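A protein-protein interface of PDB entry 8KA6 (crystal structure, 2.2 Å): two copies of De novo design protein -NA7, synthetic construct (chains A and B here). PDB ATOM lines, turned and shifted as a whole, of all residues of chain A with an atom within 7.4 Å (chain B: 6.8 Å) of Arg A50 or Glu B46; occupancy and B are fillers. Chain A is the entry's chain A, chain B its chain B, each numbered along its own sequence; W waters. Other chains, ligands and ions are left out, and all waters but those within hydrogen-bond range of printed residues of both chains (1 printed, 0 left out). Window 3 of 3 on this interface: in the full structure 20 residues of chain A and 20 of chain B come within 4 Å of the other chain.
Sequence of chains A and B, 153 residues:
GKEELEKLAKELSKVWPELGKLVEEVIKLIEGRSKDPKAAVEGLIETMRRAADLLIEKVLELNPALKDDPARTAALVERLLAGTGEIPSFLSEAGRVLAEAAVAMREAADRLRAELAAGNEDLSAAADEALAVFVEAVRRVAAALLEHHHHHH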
ATOM      1  N   LEU A  19     -34.833  11.860 -23.390  1.00  0.00           N
ATOM      2  CA  LEU A  19     -35.269  10.777 -22.515  1.00  0.00           C
ATOM      3  C   LEU A  19     -35.529   9.498 -23.298  1.00  0.00           C
ATOM      4  O   LEU A  19     -35.350   8.398 -22.761  1.00  0.00           O
ATOM      5  CB  LEU A  19     -36.520  11.196 -21.738  1.00  0.00           C
ATOM      6  CG  LEU A  19     -37.066  10.184 -20.728  1.00  0.00           C
ATOM      7  CD1 LEU A  19     -36.019   9.853 -19.671  1.00  0.00           C
ATOM      8  CD2 LEU A  19     -38.351  10.682 -20.078  1.00  0.00           C
ATOM      9  N   LYS A  21     -33.750   8.333 -25.733  1.00  0.00           N
ATOM     10  CA  LYS A  21     -32.474   7.640 -25.867  1.00  0.00           C
ATOM     11  C   LYS A  21     -32.094   6.918 -24.582  1.00  0.00           C
ATOM     12  O   LYS A  21     -31.410   5.890 -24.628  1.00  0.00           O
ATOM     13  CB  LYS A  21     -31.378   8.626 -26.271  1.00  0.00           C
ATOM     14  N   LEU A  22     -32.526   7.437 -23.428  1.00  0.00           N
ATOM     15  CA  LEU A  22     -32.281   6.741 -22.169  1.00  0.00           C
ATOM     16  C   LEU A  22     -33.138   5.486 -22.059  1.00  0.00           C
ATOM     17  O   LEU A  22     -32.696   4.473 -21.505  1.00  0.00           O
ATOM     18  CB  LEU A  22     -32.541   7.677 -20.991  1.00  0.00           C
ATOM     19  CG  LEU A  22     -31.516   8.793 -20.792  1.00  0.00           C
ATOM     20  CD1 LEU A  22     -31.943   9.713 -19.666  1.00  0.00           C
ATOM     21  CD2 LEU A  22     -30.141   8.207 -20.513  1.00  0.00           C
ATOM     22  N   GLU A  25     -31.448   2.941 -23.937  1.00  0.00           N
ATOM     23  CA  GLU A  25     -30.311   2.410 -23.192  1.00  0.00           C
ATOM     24  C   GLU A  25     -30.733   1.254 -22.296  1.00  0.00           C
ATOM     25  O   GLU A  25     -30.044   0.230 -22.223  1.00  0.00           O
ATOM     26  CB  GLU A  25     -29.658   3.514 -22.360  1.00  0.00           C
ATOM     27  CG  GLU A  25     -28.294   3.960 -22.861  1.00  0.00           C
ATOM     28  CD  GLU A  25     -27.620   4.936 -21.914  1.00  0.00           C
ATOM     29  OE1 GLU A  25     -27.431   4.587 -20.729  1.00  0.00           O
ATOM     30  OE2 GLU A  25     -27.288   6.058 -22.352  1.00  0.00           O
ATOM     31  N   LEU A  29     -29.669  -2.755 -22.295  1.00  0.00           N
ATOM     32  CA  LEU A  29     -29.212  -3.490 -21.120  1.00  0.00           C
ATOM     33  C   LEU A  29     -30.039  -4.750 -20.907  1.00  0.00           C
ATOM     34  O   LEU A  29     -29.510  -5.787 -20.489  1.00  0.00           O
ATOM     35  CB  LEU A  29     -29.275  -2.591 -19.886  1.00  0.00           C
ATOM     36  CG  LEU A  29     -28.393  -1.343 -19.915  1.00  0.00           C
ATOM     37  CD1 LEU A  29     -28.862  -0.332 -18.882  1.00  0.00           C
ATOM     38  CD2 LEU A  29     -26.936  -1.715 -19.684  1.00  0.00           C
ATOM     39  N   GLY A  43     -25.482  -1.278 -15.074  1.00  0.00           N
ATOM     40  CA  GLY A  43     -25.850  -0.355 -16.132  1.00  0.00           C
ATOM     41  C   GLY A  43     -27.220   0.258 -15.933  1.00  0.00           C
ATOM     42  O   GLY A  43     -27.449   1.410 -16.312  1.00  0.00           O
ATOM     43  N   LEU A  44     -28.147  -0.497 -15.342  1.00  0.00           N
ATOM     44  CA  LEU A  44     -29.472   0.045 -15.061  1.00  0.00           C
ATOM     45  C   LEU A  44     -29.413   1.097 -13.962  1.00  0.00           C
ATOM     46  O   LEU A  44     -30.140   2.096 -14.009  1.00  0.00           O
ATOM     47  CB  LEU A  44     -30.428  -1.083 -14.677  1.00  0.00           C
ATOM     48  CG  LEU A  44     -31.870  -0.675 -14.375  1.00  0.00           C
ATOM     49  CD1 LEU A  44     -32.490   0.011 -15.581  1.00  0.00           C
ATOM     50  CD2 LEU A  44     -32.691  -1.885 -13.957  1.00  0.00           C
ATOM     51  N   ILE A  45     -28.548   0.892 -12.966  1.00  0.00           N
ATOM     52  CA  ILE A  45     -28.385   1.878 -11.902  1.00  0.00           C
ATOM     53  C   ILE A  45     -27.836   3.183 -12.468  1.00  0.00           C
ATOM     54  O   ILE A  45     -28.277   4.274 -12.090  1.00  0.00           O
ATOM     55  CB  ILE A  45     -27.480   1.315 -10.791  1.00  0.00           C
ATOM     56  CG1 ILE A  45     -28.119   0.078 -10.159  1.00  0.00           C
ATOM     57  CG2 ILE A  45     -27.203   2.374  -9.733  1.00  0.00           C
ATOM     58  CD1 ILE A  45     -27.201  -0.667  -9.219  1.00  0.00           C
ATOM     59  N   GLU A  46     -26.870   3.090 -13.384  1.00  0.00           N
ATOM     60  CA  GLU A  46     -26.312   4.290 -14.000  1.00  0.00           C
ATOM     61  C   GLU A  46     -27.370   5.039 -14.799  1.00  0.00           C
ATOM     62  O   GLU A  46     -27.489   6.266 -14.699  1.00  0.00           O
ATOM     63  CB  GLU A  46     -25.130   3.924 -14.899  1.00  0.00           C
ATOM     64  CG  GLU A  46     -23.848   3.556 -14.169  1.00  0.00           C
ATOM     65  CD  GLU A  46     -22.688   3.343 -15.126  1.00  0.00           C
ATOM     66  OE1 GLU A  46     -22.897   3.484 -16.349  1.00  0.00           O
ATOM     67  OE2 GLU A  46     -21.570   3.035 -14.659  1.00  0.00           O
ATOM     68  N   THR A  47     -28.153   4.312 -15.600  1.00  0.00           N
ATOM     69  CA  THR A  47     -29.114   4.968 -16.481  1.00  0.00           C
ATOM     70  C   THR A  47     -30.235   5.627 -15.685  1.00  0.00           C
ATOM     71  O   THR A  47     -30.655   6.744 -16.008  1.00  0.00           O
ATOM     72  CB  THR A  47     -29.676   3.962 -17.488  1.00  0.00           C
ATOM     73  OG1 THR A  47     -28.597   3.339 -18.195  1.00  0.00           O
ATOM     74  CG2 THR A  47     -30.580   4.660 -18.494  1.00  0.00           C
ATOM     75  N   MET A  48     -30.725   4.961 -14.636  1.00  0.00           N
ATOM     76  CA  MET A  48     -31.792   5.548 -13.831  1.00  0.00           C
ATOM     77  C   MET A  48     -31.314   6.788 -13.085  1.00  0.00           C
ATOM     78  O   MET A  48     -32.093   7.727 -12.882  1.00  0.00           O
ATOM     79  CB  MET A  48     -32.350   4.516 -12.850  1.00  0.00           C
ATOM     80  CG  MET A  48     -33.000   3.306 -13.515  1.00  0.00           C
ATOM     81  SD  MET A  48     -33.785   2.170 -12.355  1.00  0.00           S
ATOM     82  CE  MET A  48     -35.144   3.175 -11.764  1.00  0.00           C
ATOM     83  N   ARG A  49     -30.047   6.811 -12.667  1.00  0.00           N
ATOM     84  CA  ARG A  49     -29.499   8.016 -12.055  1.00  0.00           C
ATOM     85  C   ARG A  49     -29.434   9.154 -13.065  1.00  0.00           C
ATOM     86  O   ARG A  49     -29.858  10.280 -12.776  1.00  0.00           O
ATOM     87  CB  ARG A  49     -28.114   7.732 -11.476  1.00  0.00           C
ATOM     88  CG  ARG A  49     -28.111   6.909 -10.199  1.00  0.00           C
ATOM     89  CD  ARG A  49     -26.686   6.581  -9.787  1.00  0.00           C
ATOM     90  NE  ARG A  49     -26.626   5.808  -8.552  1.00  0.00           N
ATOM     91  CZ  ARG A  49     -25.532   5.214  -8.095  1.00  0.00           C
ATOM     92  NH1 ARG A  49     -24.387   5.270  -8.755  1.00  0.00           N
ATOM     93  NH2 ARG A  49     -25.591   4.542  -6.948  1.00  0.00           N
ATOM     94  N   ARG A  50     -28.910   8.877 -14.262  1.00  0.00           N
ATOM     95  CA  ARG A  50     -28.857   9.901 -15.299  1.00  0.00           C
ATOM     96  C   ARG A  50     -30.250  10.298 -15.768  1.00  0.00           C
ATOM     97  O   ARG A  50     -30.465  11.454 -16.153  1.00  0.00           O
ATOM     98  CB  ARG A  50     -28.006   9.416 -16.475  1.00  0.00           C
ATOM     99  CG  ARG A  50     -26.506   9.547 -16.237  1.00  0.00           C
ATOM    100  CD  ARG A  50     -25.681   9.172 -17.466  1.00  0.00           C
ATOM    101  NE  ARG A  50     -25.567   7.730 -17.648  1.00  0.00           N
ATOM    102  CZ  ARG A  50     -26.141   7.048 -18.629  1.00  0.00           C
ATOM    103  NH1 ARG A  50     -26.874   7.649 -19.553  1.00  0.00           N
ATOM    104  NH2 ARG A  50     -25.973   5.730 -18.688  1.00  0.00           N
ATOM    105  N   ALA A  51     -31.207   9.368 -15.737  1.00  0.00           N
ATOM    106  CA  ALA A  51     -32.578   9.719 -16.087  1.00  0.00           C
ATOM    107  C   ALA A  51     -33.192  10.641 -15.041  1.00  0.00           C
ATOM    108  O   ALA A  51     -33.913  11.585 -15.385  1.00  0.00           O
ATOM    109  CB  ALA A  51     -33.420   8.456 -16.256  1.00  0.00           C
ATOM    110  N   ALA A  52     -32.915  10.386 -13.761  1.00  0.00           N
ATOM    111  CA  ALA A  52     -33.417  11.266 -12.711  1.00  0.00           C
ATOM    112  C   ALA A  52     -32.778  12.646 -12.797  1.00  0.00           C
ATOM    113  O   ALA A  52     -33.441  13.661 -12.557  1.00  0.00           O
ATOM    114  CB  ALA A  52     -33.168  10.640 -11.339  1.00  0.00           C
ATOM    115  N   ASP A  53     -31.488  12.702 -13.141  1.00  0.00           N
ATOM    116  CA  ASP A  53     -30.834  13.991 -13.348  1.00  0.00           C
ATOM    117  C   ASP A  53     -31.417  14.715 -14.554  1.00  0.00           C
ATOM    118  O   ASP A  53     -31.591  15.939 -14.526  1.00  0.00           O
ATOM    119  CB  ASP A  53     -29.328  13.796 -13.517  1.00  0.00           C
ATOM    120  CG  ASP A  53     -28.614  13.603 -12.194  1.00  0.00           C
ATOM    121  OD1 ASP A  53     -29.238  13.841 -11.140  1.00  0.00           O
ATOM    122  OD2 ASP A  53     -27.427  13.213 -12.210  1.00  0.00           O
ATOM    123  N   LEU A  54     -31.727  13.977 -15.623  1.00  0.00           N
ATOM    124  CA  LEU A  54     -32.325  14.601 -16.797  1.00  0.00           C
ATOM    125  C   LEU A  54     -33.719  15.134 -16.493  1.00  0.00           C
ATOM    126  O   LEU A  54     -34.124  16.163 -17.048  1.00  0.00           O
ATOM    127  CB  LEU A  54     -32.377  13.602 -17.953  1.00  0.00           C
ATOM    128  CG  LEU A  54     -32.760  14.170 -19.322  1.00  0.00           C
ATOM    129  CD1 LEU A  54     -31.604  14.950 -19.934  1.00  0.00           C
ATOM    130  CD2 LEU A  54     -33.231  13.069 -20.260  1.00  0.00           C
ATOM    131  N   LEU A  55     -34.461  14.457 -15.612  1.00  0.00           N
ATOM    132  CA  LEU A  55     -35.801  14.914 -15.260  1.00  0.00           C
ATOM    133  C   LEU A  55     -35.753  16.216 -14.469  1.00  0.00           C
ATOM    134  O   LEU A  55     -36.543  17.131 -14.726  1.00  0.00           O
ATOM    135  CB  LEU A  55     -36.534  13.828 -14.472  1.00  0.00           C
ATOM    136  CG  LEU A  55     -36.972  12.590 -15.259  1.00  0.00           C
ATOM    137  CD1 LEU A  55     -37.425  11.476 -14.329  1.00  0.00           C
ATOM    138  CD2 LEU A  55     -38.075  12.951 -16.233  1.00  0.00           C
ATOM    139  N   ILE A  56     -34.836  16.315 -13.502  1.00  0.00           N
ATOM    140  CA  ILE A  56     -34.701  17.544 -12.720  1.00  0.00           C
ATOM    141  C   ILE A  56     -34.323  18.709 -13.624  1.00  0.00           C
ATOM    142  O   ILE A  56     -34.835  19.826 -13.473  1.00  0.00           O
ATOM    143  CB  ILE A  56     -33.673  17.345 -11.590  1.00  0.00           C
ATOM    144  CG1 ILE A  56     -34.258  16.472 -10.478  1.00  0.00           C
ATOM    145  CG2 ILE A  56     -33.219  18.684 -11.033  1.00  0.00           C
ATOM    146  CD1 ILE A  56     -35.404  17.123  -9.731  1.00  0.00           C
ATOM    147  N   MET A 105     -37.200   7.436  -9.482  1.00  0.00           N
ATOM    148  CA  MET A 105     -36.091   6.757 -10.144  1.00  0.00           C
ATOM    149  C   MET A 105     -34.851   6.734  -9.259  1.00  0.00           C
ATOM    150  O   MET A 105     -34.111   5.744  -9.244  1.00  0.00           O
ATOM    151  CB  MET A 105     -35.775   7.431 -11.479  1.00  0.00           C
ATOM    152  CG  MET A 105     -36.859   7.291 -12.533  1.00  0.00           C
ATOM    153  SD  MET A 105     -36.301   7.907 -14.134  1.00  0.00           S
ATOM    154  CE  MET A 105     -37.791   7.752 -15.112  1.00  0.00           C
ATOM    155  N   ALA A 109     -33.134   3.383  -7.946  1.00  0.00           N
ATOM    156  CA  ALA A 109     -31.743   3.097  -8.281  1.00  0.00           C
ATOM    157  C   ALA A 109     -30.906   2.881  -7.027  1.00  0.00           C
ATOM    158  O   ALA A 109     -30.005   2.034  -7.014  1.00  0.00           O
ATOM    159  CB  ALA A 109     -31.162   4.230  -9.128  1.00  0.00           C
ATOM    160  N   VAL B  41     -18.437  18.405 -16.733  1.00  0.00           N
ATOM    161  CA  VAL B  41     -19.164  18.385 -15.467  1.00  0.00           C
ATOM    162  C   VAL B  41     -20.003  17.117 -15.356  1.00  0.00           C
ATOM    163  O   VAL B  41     -20.000  16.439 -14.321  1.00  0.00           O
ATOM    164  CB  VAL B  41     -20.030  19.649 -15.323  1.00  0.00           C
ATOM    165  CG1 VAL B  41     -21.077  19.456 -14.237  1.00  0.00           C
ATOM    166  CG2 VAL B  41     -19.156  20.857 -15.018  1.00  0.00           C
ATOM    167  N   GLU B  42     -20.737  16.781 -16.420  1.00  0.00           N
ATOM    168  CA  GLU B  42     -21.544  15.566 -16.403  1.00  0.00           C
ATOM    169  C   GLU B  42     -20.681  14.322 -16.244  1.00  0.00           C
ATOM    170  O   GLU B  42     -21.139  13.316 -15.691  1.00  0.00           O
ATOM    171  CB  GLU B  42     -22.386  15.480 -17.676  1.00  0.00           C
ATOM    172  CG  GLU B  42     -23.546  16.461 -17.702  1.00  0.00           C
ATOM    173  CD  GLU B  42     -24.042  16.745 -19.106  1.00  0.00           C
ATOM    174  OE1 GLU B  42     -23.348  16.364 -20.072  1.00  0.00           O
ATOM    175  OE2 GLU B  42     -25.124  17.355 -19.242  1.00  0.00           O
ATOM    176  N   GLY B  43     -19.433  14.370 -16.713  1.00  0.00           N
ATOM    177  CA  GLY B  43     -18.531  13.255 -16.485  1.00  0.00           C
ATOM    178  C   GLY B  43     -18.042  13.194 -15.052  1.00  0.00           C
ATOM    179  O   GLY B  43     -17.879  12.108 -14.486  1.00  0.00           O
ATOM    180  N   LEU B  44     -17.797  14.358 -14.444  1.00  0.00           N
ATOM    181  CA  LEU B  44     -17.352  14.392 -13.056  1.00  0.00           C
ATOM    182  C   LEU B  44     -18.442  13.916 -12.106  1.00  0.00           C
ATOM    183  O   LEU B  44     -18.140  13.290 -11.083  1.00  0.00           O
ATOM    184  CB  LEU B  44     -16.904  15.808 -12.687  1.00  0.00           C
ATOM    185  CG  LEU B  44     -16.461  16.031 -11.240  1.00  0.00           C
ATOM    186  CD1 LEU B  44     -15.279  15.136 -10.901  1.00  0.00           C
ATOM    187  CD2 LEU B  44     -16.118  17.495 -10.997  1.00  0.00           C
ATOM    188  N   ILE B  45     -19.706  14.204 -12.420  1.00  0.00           N
ATOM    189  CA  ILE B  45     -20.804  13.773 -11.561  1.00  0.00           C
ATOM    190  C   ILE B  45     -20.897  12.254 -11.549  1.00  0.00           C
ATOM    191  O   ILE B  45     -20.997  11.627 -10.488  1.00  0.00           O
ATOM    192  CB  ILE B  45     -22.128  14.412 -12.020  1.00  0.00           C
ATOM    193  CG1 ILE B  45     -22.057  15.936 -11.923  1.00  0.00           C
ATOM    194  CG2 ILE B  45     -23.297  13.869 -11.205  1.00  0.00           C
ATOM    195  CD1 ILE B  45     -23.256  16.633 -12.528  1.00  0.00           C
ATOM    196  N   GLU B  46     -20.858  11.640 -12.734  1.00  0.00           N
ATOM    197  CA  GLU B  46     -21.002  10.191 -12.809  1.00  0.00           C
ATOM    198  C   GLU B  46     -19.768   9.475 -12.275  1.00  0.00           C
ATOM    199  O   GLU B  46     -19.885   8.378 -11.718  1.00  0.00           O
ATOM    200  CB  GLU B  46     -21.291   9.766 -14.247  1.00  0.00           C
ATOM    201  CG  GLU B  46     -21.712   8.314 -14.375  1.00  0.00           C
ATOM    202  CD  GLU B  46     -22.384   8.014 -15.697  1.00  0.00           C
ATOM    203  OE1 GLU B  46     -22.017   8.651 -16.708  1.00  0.00           O
ATOM    204  OE2 GLU B  46     -23.286   7.150 -15.724  1.00  0.00           O
ATOM    205  N   THR B  47     -18.586  10.078 -12.426  1.00  0.00           N
ATOM    206  CA  THR B  47     -17.367   9.459 -11.913  1.00  0.00           C
ATOM    207  C   THR B  47     -17.317   9.517 -10.392  1.00  0.00           C
ATOM    208  O   THR B  47     -16.862   8.567  -9.743  1.00  0.00           O
ATOM    209  CB  THR B  47     -16.134  10.140 -12.508  1.00  0.00           C
ATOM    210  OG1 THR B  47     -16.201  10.096 -13.938  1.00  0.00           O
ATOM    211  CG2 THR B  47     -14.865   9.438 -12.045  1.00  0.00           C
ATOM    212  N   MET B  48     -17.766  10.627  -9.803  1.00  0.00           N
ATOM    213  CA  MET B  48     -17.785  10.719  -8.348  1.00  0.00           C
ATOM    214  C   MET B  48     -18.816   9.771  -7.751  1.00  0.00           C
ATOM    215  O   MET B  48     -18.604   9.217  -6.666  1.00  0.00           O
ATOM    216  CB  MET B  48     -18.059  12.158  -7.915  1.00  0.00           C
ATOM    217  CG  MET B  48     -16.891  13.101  -8.142  1.00  0.00           C
ATOM    218  SD  MET B  48     -17.327  14.796  -7.724  1.00  0.00           S
ATOM    219  CE  MET B  48     -17.644  14.634  -5.969  1.00  0.00           C
ATOM    220  N   ARG B  49     -19.936   9.566  -8.449  1.00  0.00           N
ATOM    221  CA  ARG B  49     -20.917   8.583  -8.001  1.00  0.00           C
ATOM    222  C   ARG B  49     -20.371   7.166  -8.125  1.00  0.00           C
ATOM    223  O   ARG B  49     -20.583   6.336  -7.234  1.00  0.00           O
ATOM    224  CB  ARG B  49     -22.210   8.729  -8.800  1.00  0.00           C
ATOM    225  CG  ARG B  49     -23.012   9.975  -8.469  1.00  0.00           C
ATOM    226  CD  ARG B  49     -24.194  10.125  -9.410  1.00  0.00           C
ATOM    227  NE  ARG B  49     -25.013  11.284  -9.079  1.00  0.00           N
ATOM    228  CZ  ARG B  49     -25.974  11.767  -9.855  1.00  0.00           C
ATOM    229  NH1 ARG B  49     -26.258  11.219 -11.025  1.00  0.00           N
ATOM    230  NH2 ARG B  49     -26.663  12.829  -9.449  1.00  0.00           N
ATOM    231  N   ARG B  50     -19.677   6.867  -9.228  1.00  0.00           N
ATOM    232  CA  ARG B  50     -19.017   5.570  -9.354  1.00  0.00           C
ATOM    233  C   ARG B  50     -17.980   5.375  -8.258  1.00  0.00           C
ATOM    234  O   ARG B  50     -17.803   4.262  -7.749  1.00  0.00           O
ATOM    235  CB  ARG B  50     -18.356   5.433 -10.725  1.00  0.00           C
ATOM    236  CG  ARG B  50     -19.311   5.200 -11.880  1.00  0.00           C
ATOM    237  CD  ARG B  50     -18.724   4.182 -12.844  1.00  0.00           C
ATOM    238  NE  ARG B  50     -19.086   4.451 -14.231  1.00  0.00           N
ATOM    239  CZ  ARG B  50     -18.355   5.177 -15.064  1.00  0.00           C
ATOM    240  NH1 ARG B  50     -17.217   5.733 -14.681  1.00  0.00           N
ATOM    241  NH2 ARG B  50     -18.775   5.351 -16.314  1.00  0.00           N
ATOM    242  N   ALA B  51     -17.277   6.446  -7.885  1.00  0.00           N
ATOM    243  CA  ALA B  51     -16.313   6.349  -6.794  1.00  0.00           C
ATOM    244  C   ALA B  51     -17.010   6.041  -5.475  1.00  0.00           C
ATOM    245  O   ALA B  51     -16.485   5.291  -4.645  1.00  0.00           O
ATOM    246  CB  ALA B  51     -15.509   7.642  -6.690  1.00  0.00           C
ATOM    247  N   ALA B 109     -21.688  15.327  -5.466  1.00  0.00           N
ATOM    248  CA  ALA B 109     -22.116  15.050  -6.834  1.00  0.00           C
ATOM    249  C   ALA B 109     -23.517  15.587  -7.093  1.00  0.00           C
ATOM    250  O   ALA B 109     -23.784  16.156  -8.158  1.00  0.00           O
ATOM    251  CB  ALA B 109     -22.055  13.547  -7.108  1.00  0.00           C
ATOM    252  N   ARG B 113     -24.656  18.624  -9.608  1.00  0.00           N
ATOM    253  CA  ARG B 113     -25.786  18.439 -10.514  1.00  0.00           C
ATOM    254  C   ARG B 113     -26.810  19.555 -10.344  1.00  0.00           C
ATOM    255  O   ARG B 113     -27.356  20.062 -11.331  1.00  0.00           O
ATOM    256  CB  ARG B 113     -26.421  17.066 -10.279  1.00  0.00           C
ATOM    257  CG  ARG B 113     -27.846  16.890 -10.810  1.00  0.00           C
ATOM    258  CD  ARG B 113     -27.959  17.140 -12.311  1.00  0.00           C
ATOM    259  NE  ARG B 113     -26.966  16.407 -13.085  1.00  0.00           N
ATOM    260  CZ  ARG B 113     -26.785  16.555 -14.390  1.00  0.00           C
ATOM    261  NH1 ARG B 113     -27.517  17.399 -15.098  1.00  0.00           N
ATOM    262  NH2 ARG B 113     -25.842  15.841 -14.999  1.00  0.00           N
HETATM  263  O   HOH W   1     -23.084   6.272  -5.802  1.00  0.00           O
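Of the 21 printed residues of chain A, 4 touch a printed residue of chain B.
Among the printed residues, 6 pairs touch across the chains.
Among the printed residues, Asp or Glu carboxylates within 4 Å of a Lys or Arg side-chain nitrogen of the other chain: Glu A46 with Arg B50, Arg A50 with Glu B46, Asp A53 with Arg B49 and Asp A53 with Arg B113.
OE2 of Glu B46 touches OE1 of Glu A46 (3.7 Å).
Arg B49 touches Arg A49 (NH1 to CB, 3.98 Å).
Water W1 lies within hydrogen-bond range of the backbone carbonyl oxygen of Arg B49 (2.9 Å) and the guanidinium group of Arg A49 (3.3 Å).
Arg A50 touches one residue of chain B.
Glu B46 touches two residues of chain A.
Of the printed residues of chain B, Arg A49 touches Arg B49 (3.98 Å).
Of the printed residues of chain A, Arg B50 touches Glu A46 (2.9 Å).
Printed residues of chain B within 4 Å of Glu A46: Glu B46 (3.7 Å) and Arg B50 (2.9 Å).
Ala B109 touches none of the printed residues of chain A.
Leu A22 touches none of the printed residues of chain B.
The side-chain carboxylate of Asp A53 lies within salt-bridge range of the guanidinium group of Arg B49, at 2.6 Å.
The side-chain carboxylate of Glu A46 is in salt-bridge range of the guanidinium group of Arg B50, at 2.9 Å.
The guanidinium group (NE) of Arg A50 lies within salt-bridge range of the side-chain carboxylate (OE2) of Glu B46.
The side-chain carboxylate (OD2) of Asp A53 is in salt-bridge range of the guanidinium group (NE) of Arg B113 (3.3 Å).
OE1 of Glu A25 lies within salt-bridge range of NH2 of Arg A50.
Glu A46 touches its own counterpart, Glu B46.
Glu A46 touches Arg B50, and with the chains exchanged Arg A50 touches Glu B46.
Arg B49 touches its own counterpart, Arg A49.
Of the 6 pairs that touch across the chains among the printed residues, 4 have their exchanged pair printed and touching as well.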
